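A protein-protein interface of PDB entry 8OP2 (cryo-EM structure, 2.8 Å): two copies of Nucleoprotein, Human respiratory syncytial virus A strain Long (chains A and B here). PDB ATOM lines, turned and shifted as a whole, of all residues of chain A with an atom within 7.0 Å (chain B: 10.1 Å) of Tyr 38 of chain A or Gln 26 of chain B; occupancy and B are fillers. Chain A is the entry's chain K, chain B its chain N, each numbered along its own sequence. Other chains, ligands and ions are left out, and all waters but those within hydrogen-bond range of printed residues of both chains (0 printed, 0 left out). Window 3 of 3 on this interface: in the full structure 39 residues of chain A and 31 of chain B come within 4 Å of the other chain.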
ATOM      1  N   PRO A  36       7.066   5.491   9.838  1.00  0.00           N
ATOM      2  CA  PRO A  36       7.961   5.490   8.682  1.00  0.00           C
ATOM      3  C   PRO A  36       7.244   5.049   7.417  1.00  0.00           C
ATOM      4  O   PRO A  36       6.277   4.288   7.446  1.00  0.00           O
ATOM      5  CB  PRO A  36       9.046   4.483   9.073  1.00  0.00           C
ATOM      6  CG  PRO A  36       8.397   3.593  10.053  1.00  0.00           C
ATOM      7  CD  PRO A  36       7.400   4.426  10.797  1.00  0.00           C
ATOM      8  N   ASN A  37       7.740   5.547   6.293  1.00  0.00           N
ATOM      9  CA  ASN A  37       7.194   5.245   4.978  1.00  0.00           C
ATOM     10  C   ASN A  37       8.160   4.317   4.245  1.00  0.00           C
ATOM     11  O   ASN A  37       9.154   3.854   4.806  1.00  0.00           O
ATOM     12  CB  ASN A  37       6.934   6.535   4.200  1.00  0.00           C
ATOM     13  CG  ASN A  37       5.848   6.379   3.159  1.00  0.00           C
ATOM     14  OD1 ASN A  37       4.775   5.857   3.444  1.00  0.00           O
ATOM     15  ND2 ASN A  37       6.120   6.839   1.947  1.00  0.00           N
ATOM     16  N   TYR A  38       7.856   4.043   2.974  1.00  0.00           N
ATOM     17  CA  TYR A  38       8.718   3.186   2.169  1.00  0.00           C
ATOM     18  C   TYR A  38      10.107   3.777   1.990  1.00  0.00           C
ATOM     19  O   TYR A  38      11.043   3.043   1.654  1.00  0.00           O
ATOM     20  CB  TYR A  38       8.092   2.947   0.798  1.00  0.00           C
ATOM     21  CG  TYR A  38       6.667   2.460   0.835  1.00  0.00           C
ATOM     22  CD1 TYR A  38       6.330   1.287   1.487  1.00  0.00           C
ATOM     23  CD2 TYR A  38       5.658   3.171   0.206  1.00  0.00           C
ATOM     24  CE1 TYR A  38       5.031   0.841   1.516  1.00  0.00           C
ATOM     25  CE2 TYR A  38       4.357   2.731   0.233  1.00  0.00           C
ATOM     26  CZ  TYR A  38       4.049   1.566   0.888  1.00  0.00           C
ATOM     27  OH  TYR A  38       2.749   1.125   0.914  1.00  0.00           O
ATOM     28  N   ASP A  39      10.258   5.082   2.205  1.00  0.00           N
ATOM     29  CA  ASP A  39      11.522   5.754   1.927  1.00  0.00           C
ATOM     30  C   ASP A  39      12.646   5.224   2.805  1.00  0.00           C
ATOM     31  O   ASP A  39      13.766   5.013   2.328  1.00  0.00           O
ATOM     32  CB  ASP A  39      11.352   7.255   2.141  1.00  0.00           C
ATOM     33  CG  ASP A  39      10.452   7.884   1.108  1.00  0.00           C
ATOM     34  OD1 ASP A  39      10.401   7.368  -0.026  1.00  0.00           O
ATOM     35  OD2 ASP A  39       9.792   8.892   1.432  1.00  0.00           O
ATOM     36  N   VAL A  40      12.369   5.007   4.089  1.00  0.00           N
ATOM     37  CA  VAL A  40      13.398   4.679   5.066  1.00  0.00           C
ATOM     38  C   VAL A  40      13.466   3.182   5.344  1.00  0.00           C
ATOM     39  O   VAL A  40      14.099   2.765   6.320  1.00  0.00           O
ATOM     40  CB  VAL A  40      13.180   5.470   6.360  1.00  0.00           C
ATOM     41  CG1 VAL A  40      13.412   6.945   6.108  1.00  0.00           C
ATOM     42  CG2 VAL A  40      11.778   5.244   6.873  1.00  0.00           C
ATOM     43  N   GLN A  41      12.823   2.365   4.509  1.00  0.00           N
ATOM     44  CA  GLN A  41      12.883   0.918   4.684  1.00  0.00           C
ATOM     45  C   GLN A  41      14.311   0.409   4.566  1.00  0.00           C
ATOM     46  O   GLN A  41      14.736  -0.455   5.342  1.00  0.00           O
ATOM     47  CB  GLN A  41      11.987   0.242   3.650  1.00  0.00           C
ATOM     48  CG  GLN A  41      11.515  -1.137   4.032  1.00  0.00           C
ATOM     49  CD  GLN A  41      10.679  -1.769   2.948  1.00  0.00           C
ATOM     50  OE1 GLN A  41      10.927  -2.900   2.541  1.00  0.00           O
ATOM     51  NE2 GLN A  41       9.685  -1.039   2.469  1.00  0.00           N
ATOM     52  N   LYS A  42      15.068   0.939   3.605  1.00  0.00           N
ATOM     53  CA  LYS A  42      16.460   0.537   3.443  1.00  0.00           C
ATOM     54  C   LYS A  42      17.279   0.872   4.680  1.00  0.00           C
ATOM     55  O   LYS A  42      18.098   0.064   5.127  1.00  0.00           O
ATOM     56  CB  LYS A  42      17.056   1.219   2.214  1.00  0.00           C
ATOM     57  CG  LYS A  42      16.457   0.768   0.898  1.00  0.00           C
ATOM     58  CD  LYS A  42      17.190   1.387  -0.282  1.00  0.00           C
ATOM     59  CE  LYS A  42      16.570   0.967  -1.606  1.00  0.00           C
ATOM     60  NZ  LYS A  42      17.532   1.088  -2.732  1.00  0.00           N
ATOM     61  N   MET A  71       6.348  -1.485  10.173  1.00  0.00           N
ATOM     62  CA  MET A  71       5.535  -0.334   9.802  1.00  0.00           C
ATOM     63  C   MET A  71       6.024   0.341   8.529  1.00  0.00           C
ATOM     64  O   MET A  71       5.208   0.892   7.788  1.00  0.00           O
ATOM     65  CB  MET A  71       5.494   0.659  10.961  1.00  0.00           C
ATOM     66  CG  MET A  71       4.758   0.118  12.170  1.00  0.00           C
ATOM     67  SD  MET A  71       4.511   1.323  13.476  1.00  0.00           S
ATOM     68  CE  MET A  71       6.007   2.272  13.308  1.00  0.00           C
ATOM     69  N   SER A  72       7.330   0.316   8.262  1.00  0.00           N
ATOM     70  CA  SER A  72       7.845   0.868   7.013  1.00  0.00           C
ATOM     71  C   SER A  72       7.508  -0.029   5.831  1.00  0.00           C
ATOM     72  O   SER A  72       7.291   0.459   4.718  1.00  0.00           O
ATOM     73  CB  SER A  72       9.353   1.070   7.108  1.00  0.00           C
ATOM     74  OG  SER A  72      10.012  -0.168   7.265  1.00  0.00           O
ATOM     75  N   ARG A  73       7.481  -1.346   6.047  1.00  0.00           N
ATOM     76  CA  ARG A  73       7.009  -2.243   4.997  1.00  0.00           C
ATOM     77  C   ARG A  73       5.539  -2.008   4.685  1.00  0.00           C
ATOM     78  O   ARG A  73       5.137  -2.034   3.518  1.00  0.00           O
ATOM     79  CB  ARG A  73       7.233  -3.698   5.392  1.00  0.00           C
ATOM     80  CG  ARG A  73       8.630  -4.206   5.162  1.00  0.00           C
ATOM     81  CD  ARG A  73       8.589  -5.666   4.789  1.00  0.00           C
ATOM     82  NE  ARG A  73       9.791  -6.095   4.089  1.00  0.00           N
ATOM     83  CZ  ARG A  73       9.914  -7.272   3.490  1.00  0.00           C
ATOM     84  NH1 ARG A  73       8.901  -8.124   3.500  1.00  0.00           N
ATOM     85  NH2 ARG A  73      11.041  -7.595   2.877  1.00  0.00           N
ATOM     86  N   LEU A  74       4.715  -1.803   5.714  1.00  0.00           N
ATOM     87  CA  LEU A  74       3.300  -1.529   5.475  1.00  0.00           C
ATOM     88  C   LEU A  74       3.114  -0.208   4.743  1.00  0.00           C
ATOM     89  O   LEU A  74       2.239  -0.082   3.880  1.00  0.00           O
ATOM     90  CB  LEU A  74       2.535  -1.510   6.798  1.00  0.00           C
ATOM     91  CG  LEU A  74       2.045  -2.828   7.393  1.00  0.00           C
ATOM     92  CD1 LEU A  74       1.720  -2.644   8.857  1.00  0.00           C
ATOM     93  CD2 LEU A  74       0.826  -3.339   6.656  1.00  0.00           C
ATOM     94  N   GLY A  75       3.932   0.785   5.070  1.00  0.00           N
ATOM     95  CA  GLY A  75       3.779   2.132   4.577  1.00  0.00           C
ATOM     96  C   GLY A  75       3.029   3.006   5.567  1.00  0.00           C
ATOM     97  O   GLY A  75       2.298   2.528   6.433  1.00  0.00           O
ATOM     98  N   ARG A  76       3.232   4.317   5.442  1.00  0.00           N
ATOM     99  CA  ARG A  76       2.617   5.250   6.383  1.00  0.00           C
ATOM    100  C   ARG A  76       1.099   5.270   6.242  1.00  0.00           C
ATOM    101  O   ARG A  76       0.376   5.315   7.243  1.00  0.00           O
ATOM    102  CB  ARG A  76       3.196   6.651   6.198  1.00  0.00           C
ATOM    103  CG  ARG A  76       2.658   7.661   7.190  1.00  0.00           C
ATOM    104  CD  ARG A  76       3.148   9.068   6.911  1.00  0.00           C
ATOM    105  NE  ARG A  76       2.301  10.058   7.580  1.00  0.00           N
ATOM    106  CZ  ARG A  76       2.753  11.001   8.398  1.00  0.00           C
ATOM    107  NH1 ARG A  76       4.045  11.085   8.665  1.00  0.00           N
ATOM    108  NH2 ARG A  76       1.905  11.853   8.960  1.00  0.00           N
ATOM    109  N   GLU A  77       0.598   5.247   5.004  1.00  0.00           N
ATOM    110  CA  GLU A  77      -0.848   5.275   4.800  1.00  0.00           C
ATOM    111  C   GLU A  77      -1.508   4.077   5.473  1.00  0.00           C
ATOM    112  O   GLU A  77      -2.468   4.237   6.237  1.00  0.00           O
ATOM    113  CB  GLU A  77      -1.192   5.286   3.303  1.00  0.00           C
ATOM    114  CG  GLU A  77      -0.583   6.329   2.309  1.00  0.00           C
ATOM    115  CD  GLU A  77       0.614   7.162   2.766  1.00  0.00           C
ATOM    116  OE1 GLU A  77       1.368   6.773   3.676  1.00  0.00           O
ATOM    117  OE2 GLU A  77       0.799   8.255   2.192  1.00  0.00           O
ATOM    118  N   ASP A  78      -0.999   2.874   5.211  1.00  0.00           N
ATOM    119  CA  ASP A  78      -1.614   1.677   5.774  1.00  0.00           C
ATOM    120  C   ASP A  78      -1.411   1.589   7.278  1.00  0.00           C
ATOM    121  O   ASP A  78      -2.291   1.106   7.992  1.00  0.00           O
ATOM    122  CB  ASP A  78      -1.078   0.427   5.085  1.00  0.00           C
ATOM    123  CG  ASP A  78      -1.883   0.049   3.863  1.00  0.00           C
ATOM    124  OD1 ASP A  78      -2.925   0.689   3.615  1.00  0.00           O
ATOM    125  OD2 ASP A  78      -1.476  -0.886   3.145  1.00  0.00           O
ATOM    126  N   THR A 233       1.285 -11.891   0.088  1.00  0.00           N
ATOM    127  CA  THR A 233       2.075 -11.576  -1.088  1.00  0.00           C
ATOM    128  C   THR A 233       2.110 -12.763  -2.043  1.00  0.00           C
ATOM    129  O   THR A 233       1.788 -13.898  -1.688  1.00  0.00           O
ATOM    130  CB  THR A 233       3.496 -11.171  -0.697  1.00  0.00           C
ATOM    131  OG1 THR A 233       4.030 -12.124   0.226  1.00  0.00           O
ATOM    132  CG2 THR A 233       3.502  -9.802  -0.057  1.00  0.00           C
ATOM    133  N   TYR B  23      -4.894  -4.564   3.865  1.00  0.00           N
ATOM    134  CA  TYR B  23      -3.678  -3.768   3.848  1.00  0.00           C
ATOM    135  C   TYR B  23      -2.614  -4.530   3.075  1.00  0.00           C
ATOM    136  O   TYR B  23      -2.628  -5.763   3.044  1.00  0.00           O
ATOM    137  CB  TYR B  23      -3.188  -3.457   5.262  1.00  0.00           C
ATOM    138  CG  TYR B  23      -4.292  -3.081   6.220  1.00  0.00           C
ATOM    139  CD1 TYR B  23      -4.916  -1.846   6.138  1.00  0.00           C
ATOM    140  CD2 TYR B  23      -4.717  -3.965   7.198  1.00  0.00           C
ATOM    141  CE1 TYR B  23      -5.927  -1.501   7.009  1.00  0.00           C
ATOM    142  CE2 TYR B  23      -5.729  -3.628   8.071  1.00  0.00           C
ATOM    143  CZ  TYR B  23      -6.329  -2.396   7.972  1.00  0.00           C
ATOM    144  OH  TYR B  23      -7.336  -2.058   8.842  1.00  0.00           O
ATOM    145  N   THR B  24      -1.703  -3.796   2.443  1.00  0.00           N
ATOM    146  CA  THR B  24      -0.668  -4.390   1.609  1.00  0.00           C
ATOM    147  C   THR B  24       0.698  -3.844   1.990  1.00  0.00           C
ATOM    148  O   THR B  24       0.836  -2.685   2.387  1.00  0.00           O
ATOM    149  CB  THR B  24      -0.915  -4.122   0.119  1.00  0.00           C
ATOM    150  OG1 THR B  24      -0.855  -2.714  -0.131  1.00  0.00           O
ATOM    151  CG2 THR B  24      -2.269  -4.651  -0.310  1.00  0.00           C
ATOM    152  N   ILE B  25       1.707  -4.693   1.854  1.00  0.00           N
ATOM    153  CA  ILE B  25       3.089  -4.284   2.036  1.00  0.00           C
ATOM    154  C   ILE B  25       3.694  -3.976   0.674  1.00  0.00           C
ATOM    155  O   ILE B  25       3.171  -4.364  -0.372  1.00  0.00           O
ATOM    156  CB  ILE B  25       3.917  -5.353   2.772  1.00  0.00           C
ATOM    157  CG1 ILE B  25       4.105  -6.575   1.876  1.00  0.00           C
ATOM    158  CG2 ILE B  25       3.259  -5.734   4.078  1.00  0.00           C
ATOM    159  CD1 ILE B  25       5.324  -7.379   2.200  1.00  0.00           C
ATOM    160  N   GLN B  26       4.818  -3.266   0.688  1.00  0.00           N
ATOM    161  CA  GLN B  26       5.527  -2.921  -0.540  1.00  0.00           C
ATOM    162  C   GLN B  26       7.017  -2.956  -0.243  1.00  0.00           C
ATOM    163  O   GLN B  26       7.536  -2.068   0.436  1.00  0.00           O
ATOM    164  CB  GLN B  26       5.094  -1.554  -1.057  1.00  0.00           C
ATOM    165  CG  GLN B  26       5.853  -1.090  -2.279  1.00  0.00           C
ATOM    166  CD  GLN B  26       5.295   0.190  -2.857  1.00  0.00           C
ATOM    167  OE1 GLN B  26       4.252   0.676  -2.421  1.00  0.00           O
ATOM    168  NE2 GLN B  26       6.003   0.760  -3.823  1.00  0.00           N
ATOM    169  N   ARG B  27       7.695  -3.977  -0.750  1.00  0.00           N
ATOM    170  CA  ARG B  27       9.104  -4.196  -0.481  1.00  0.00           C
ATOM    171  C   ARG B  27       9.963  -3.285  -1.352  1.00  0.00           C
ATOM    172  O   ARG B  27       9.518  -2.742  -2.363  1.00  0.00           O
ATOM    173  CB  ARG B  27       9.460  -5.662  -0.705  1.00  0.00           C
ATOM    174  CG  ARG B  27       8.831  -6.599   0.298  1.00  0.00           C
ATOM    175  CD  ARG B  27       8.816  -8.031  -0.191  1.00  0.00           C
ATOM    176  NE  ARG B  27       7.813  -8.245  -1.226  1.00  0.00           N
ATOM    177  CZ  ARG B  27       7.369  -9.439  -1.595  1.00  0.00           C
ATOM    178  NH1 ARG B  27       7.837 -10.530  -1.013  1.00  0.00           N
ATOM    179  NH2 ARG B  27       6.454  -9.541  -2.546  1.00  0.00           N
ATOM    180  N   SER B  28      11.220  -3.120  -0.959  1.00  0.00           N
ATOM    181  CA  SER B  28      12.181  -2.323  -1.708  1.00  0.00           C
ATOM    182  C   SER B  28      13.296  -3.232  -2.194  1.00  0.00           C
ATOM    183  O   SER B  28      13.991  -3.854  -1.385  1.00  0.00           O
ATOM    184  CB  SER B  28      12.751  -1.194  -0.855  1.00  0.00           C
ATOM    185  OG  SER B  28      11.768  -0.210  -0.608  1.00  0.00           O
ATOM    186  N   THR B  29      13.468  -3.304  -3.510  1.00  0.00           N
ATOM    187  CA  THR B  29      14.449  -4.218  -4.073  1.00  0.00           C
ATOM    188  C   THR B  29      15.876  -3.851  -3.702  1.00  0.00           C
ATOM    189  O   THR B  29      16.743  -4.731  -3.693  1.00  0.00           O
ATOM    190  CB  THR B  29      14.325  -4.252  -5.592  1.00  0.00           C
ATOM    191  OG1 THR B  29      14.431  -2.919  -6.099  1.00  0.00           O
ATOM    192  CG2 THR B  29      12.967  -4.797  -5.982  1.00  0.00           C
ATOM    193  N   GLY B  30      16.138  -2.578  -3.404  1.00  0.00           N
ATOM    194  CA  GLY B  30      17.487  -2.110  -3.141  1.00  0.00           C
ATOM    195  C   GLY B  30      18.177  -1.529  -4.366  1.00  0.00           C
ATOM    196  O   GLY B  30      17.986  -0.362  -4.720  1.00  0.00           O
ATOM    197  N   ILE B  80       7.594  -3.968 -15.558  1.00  0.00           N
ATOM    198  CA  ILE B  80       7.267  -3.044 -14.479  1.00  0.00           C
ATOM    199  C   ILE B  80       5.978  -3.469 -13.793  1.00  0.00           C
ATOM    200  O   ILE B  80       5.887  -3.475 -12.559  1.00  0.00           O
ATOM    201  CB  ILE B  80       7.182  -1.608 -15.022  1.00  0.00           C
ATOM    202  CG1 ILE B  80       8.576  -1.086 -15.361  1.00  0.00           C
ATOM    203  CG2 ILE B  80       6.503  -0.695 -14.029  1.00  0.00           C
ATOM    204  CD1 ILE B  80       8.580   0.290 -15.971  1.00  0.00           C
ATOM    205  N   LEU B  83       6.558  -6.383 -11.531  1.00  0.00           N
ATOM    206  CA  LEU B  83       7.258  -6.022 -10.302  1.00  0.00           C
ATOM    207  C   LEU B  83       6.337  -5.308  -9.320  1.00  0.00           C
ATOM    208  O   LEU B  83       6.415  -5.548  -8.111  1.00  0.00           O
ATOM    209  CB  LEU B  83       8.481  -5.172 -10.622  1.00  0.00           C
ATOM    210  CG  LEU B  83       9.615  -5.996 -11.227  1.00  0.00           C
ATOM    211  CD1 LEU B  83      10.677  -5.096 -11.814  1.00  0.00           C
ATOM    212  CD2 LEU B  83      10.207  -6.931 -10.192  1.00  0.00           C
ATOM    213  N   ARG B  84       5.468  -4.420  -9.808  1.00  0.00           N
ATOM    214  CA  ARG B  84       4.478  -3.817  -8.916  1.00  0.00           C
ATOM    215  C   ARG B  84       3.522  -4.856  -8.347  1.00  0.00           C
ATOM    216  O   ARG B  84       3.271  -4.873  -7.137  1.00  0.00           O
ATOM    217  CB  ARG B  84       3.699  -2.709  -9.621  1.00  0.00           C
ATOM    218  CG  ARG B  84       4.374  -1.345  -9.629  1.00  0.00           C
ATOM    219  CD  ARG B  84       5.425  -1.214 -10.695  1.00  0.00           C
ATOM    220  NE  ARG B  84       6.021   0.118 -10.771  1.00  0.00           N
ATOM    221  CZ  ARG B  84       5.363   1.226 -11.103  1.00  0.00           C
ATOM    222  NH1 ARG B  84       4.074   1.179 -11.412  1.00  0.00           N
ATOM    223  NH2 ARG B  84       6.002   2.385 -11.145  1.00  0.00           N
ATOM    224  N   ASP B  85       2.969  -5.725  -9.197  1.00  0.00           N
ATOM    225  CA  ASP B  85       2.002  -6.706  -8.716  1.00  0.00           C
ATOM    226  C   ASP B  85       2.619  -7.660  -7.704  1.00  0.00           C
ATOM    227  O   ASP B  85       1.918  -8.157  -6.817  1.00  0.00           O
ATOM    228  CB  ASP B  85       1.416  -7.489  -9.886  1.00  0.00           C
ATOM    229  CG  ASP B  85       0.516  -6.644 -10.757  1.00  0.00           C
ATOM    230  OD1 ASP B  85       0.141  -5.536 -10.324  1.00  0.00           O
ATOM    231  OD2 ASP B  85       0.176  -7.090 -11.872  1.00  0.00           O
ATOM    232  N   ALA B  86       3.917  -7.934  -7.818  1.00  0.00           N
ATOM    233  CA  ALA B  86       4.589  -8.745  -6.816  1.00  0.00           C
ATOM    234  C   ALA B  86       4.807  -7.991  -5.515  1.00  0.00           C
ATOM    235  O   ALA B  86       5.211  -8.602  -4.522  1.00  0.00           O
ATOM    236  CB  ALA B  86       5.927  -9.248  -7.354  1.00  0.00           C
ATOM    237  N   GLY B  87       4.551  -6.686  -5.496  1.00  0.00           N
ATOM    238  CA  GLY B  87       4.715  -5.894  -4.295  1.00  0.00           C
ATOM    239  C   GLY B  87       6.139  -5.435  -4.077  1.00  0.00           C
ATOM    240  O   GLY B  87       6.727  -5.700  -3.025  1.00  0.00           O
ATOM    241  N   TYR B  88       6.707  -4.749  -5.062  1.00  0.00           N
ATOM    242  CA  TYR B  88       8.074  -4.261  -4.990  1.00  0.00           C
ATOM    243  C   TYR B  88       8.120  -2.785  -5.348  1.00  0.00           C
ATOM    244  O   TYR B  88       7.359  -2.319  -6.200  1.00  0.00           O
ATOM    245  CB  TYR B  88       9.005  -5.037  -5.928  1.00  0.00           C
ATOM    246  CG  TYR B  88       9.361  -6.426  -5.459  1.00  0.00           C
ATOM    247  CD1 TYR B  88      10.335  -6.622  -4.495  1.00  0.00           C
ATOM    248  CD2 TYR B  88       8.732  -7.541  -5.986  1.00  0.00           C
ATOM    249  CE1 TYR B  88      10.667  -7.886  -4.067  1.00  0.00           C
ATOM    250  CE2 TYR B  88       9.060  -8.809  -5.562  1.00  0.00           C
ATOM    251  CZ  TYR B  88      10.025  -8.975  -4.603  1.00  0.00           C
ATOM    252  OH  TYR B  88      10.350 -10.241  -4.179  1.00  0.00           O
ATOM    253  N   HIS B  89       9.009  -2.056  -4.684  1.00  0.00           N
ATOM    254  CA  HIS B  89       9.386  -0.717  -5.112  1.00  0.00           C
ATOM    255  C   HIS B  89      10.604  -0.837  -6.013  1.00  0.00           C
ATOM    256  O   HIS B  89      11.661  -1.305  -5.577  1.00  0.00           O
ATOM    257  CB  HIS B  89       9.686   0.187  -3.920  1.00  0.00           C
ATOM    258  CG  HIS B  89       9.801   1.634  -4.282  1.00  0.00           C
ATOM    259  ND1 HIS B  89      11.012   2.241  -4.529  1.00  0.00           N
ATOM    260  CD2 HIS B  89       8.858   2.588  -4.460  1.00  0.00           C
ATOM    261  CE1 HIS B  89      10.812   3.510  -4.836  1.00  0.00           C
ATOM    262  NE2 HIS B  89       9.512   3.745  -4.802  1.00  0.00           N
ATOM    263  N   VAL B  90      10.458  -0.421  -7.265  1.00  0.00           N
ATOM    264  CA  VAL B  90      11.468  -0.652  -8.285  1.00  0.00           C
ATOM    265  C   VAL B  90      11.906   0.677  -8.876  1.00  0.00           C
ATOM    266  O   VAL B  90      11.077   1.544  -9.177  1.00  0.00           O
ATOM    267  CB  VAL B  90      10.955  -1.601  -9.385  1.00  0.00           C
ATOM    268  CG1 VAL B  90      10.873  -3.015  -8.848  1.00  0.00           C
ATOM    269  CG2 VAL B  90       9.596  -1.144  -9.889  1.00  0.00           C
ATOM    270  N   LYS B  91      13.215   0.836  -9.021  1.00  0.00           N
ATOM    271  CA  LYS B  91      13.809   1.947  -9.757  1.00  0.00           C
ATOM    272  C   LYS B  91      13.966   1.477 -11.198  1.00  0.00           C
ATOM    273  O   LYS B  91      14.933   0.802 -11.548  1.00  0.00           O
ATOM    274  CB  LYS B  91      15.141   2.354  -9.144  1.00  0.00           C
ATOM    275  CG  LYS B  91      15.829   3.497  -9.857  1.00  0.00           C
ATOM    276  CD  LYS B  91      15.057   4.788  -9.706  1.00  0.00           C
ATOM    277  CE  LYS B  91      15.833   5.948 -10.297  1.00  0.00           C
ATOM    278  NZ  LYS B  91      15.969   5.817 -11.773  1.00  0.00           N
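N of His 89 of chain B sits at hydrogen-bond distance from O of Arg 27 of chain B, 2.5 Å away.
O of Gly 87 of chain B is in hydrogen-bond range of N of Arg 27 of chain B.
The guanidinium group of Arg 27 of chain B sits at hydrogen-bond distance from the backbone carbonyl oxygen of Ala 86 of chain B (2.5 Å).
OH of Tyr 38 of chain A sits at hydrogen-bond distance from O of Leu 74 of chain A (3.2 Å).
Gln 26 of chain B touches Tyr 38 of chain A (OE1 to CE2, 3.4 Å).
Gln 41 of chain A touches Arg 27 of chain B (OE1 to CA, 3.8 Å).
Gln 41 of chain A touches Ser 28 of chain B.
Ile 25 of chain B touches Arg 73 of chain A.
Arg 27 of chain B touches Arg 73 of chain A (CG to CZ, 3.4 Å).
Asp 78 of chain A touches Tyr 23 of chain B.
Ile 25 of chain B touches Thr 233 of chain A (CD1 to CG2, 3.8 Å).
NH2 of Arg 27 of chain B touches CB of Thr 233 of chain A, 3.9 Å away.
The side-chain carboxylate (OD2) of Asp 78 of chain A lies within hydrogen-bond range of the backbone NH (N) of Thr 24 of chain B (3.0 Å).
The backbone NH (N) of Gln 26 of chain B lies within hydrogen-bond range of the backbone carbonyl oxygen (O) of Arg 73 of chain A (3.1 Å).
NE2 of Gln 41 of chain A sits at hydrogen-bond distance from O of Gln 26 of chain B, 3.1 Å away.
The backbone carbonyl oxygen (O) of Thr 24 of chain B lies close to the backbone carbonyl oxygen (O) of Leu 74 of chain A.
The side-chain amino group (NZ) of Lys 42 of chain A lies within hydrogen-bond range of the backbone carbonyl oxygen (O) of Gly 30 of chain B (2.5 Å).
No position is printed for both chains.
No residue of chain B comes within 4 Å of Asn 37 of chain A.
Tyr 38 of chain A touches one residue of chain B.
No residue of chain B comes within 4 Å of Asp 39 of chain A.
No residue of chain B comes within 4 Å of Gly 75 of chain A.
Printed residues of chain A within 4 Å of Tyr 23 of chain B: Asp 78 (3.7 Å).
Printed residues of chain A within 4 Å of Ile 25 of chain B: Arg 73 and Thr 233.
Gln 26 of chain B touches just these residues of chain A: Tyr 38, Gln 41 and Arg 73.
Of the printed residues of chain A, Arg 27 of chain B touches Gln 41 (3.8 Å), Arg 73 (3.4 Å) and Thr 233 (3.9 Å).
The nearest residue of chain B that does not touch Tyr 38 of chain A is Ser 28 of chain B (4.03 Å).
Of the 18 printed residues of chain B, 7 touch a printed residue of chain A.
Printed residues of chain A that touch a printed residue of chain B: Tyr 38, Gln 41, Lys 42, Arg 73, Leu 74, Asp 78 and Thr 233.
Among the printed residues, no Asp or Glu carboxylate lies within 4 Å of a Lys or Arg side-chain nitrogen of the other chain.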
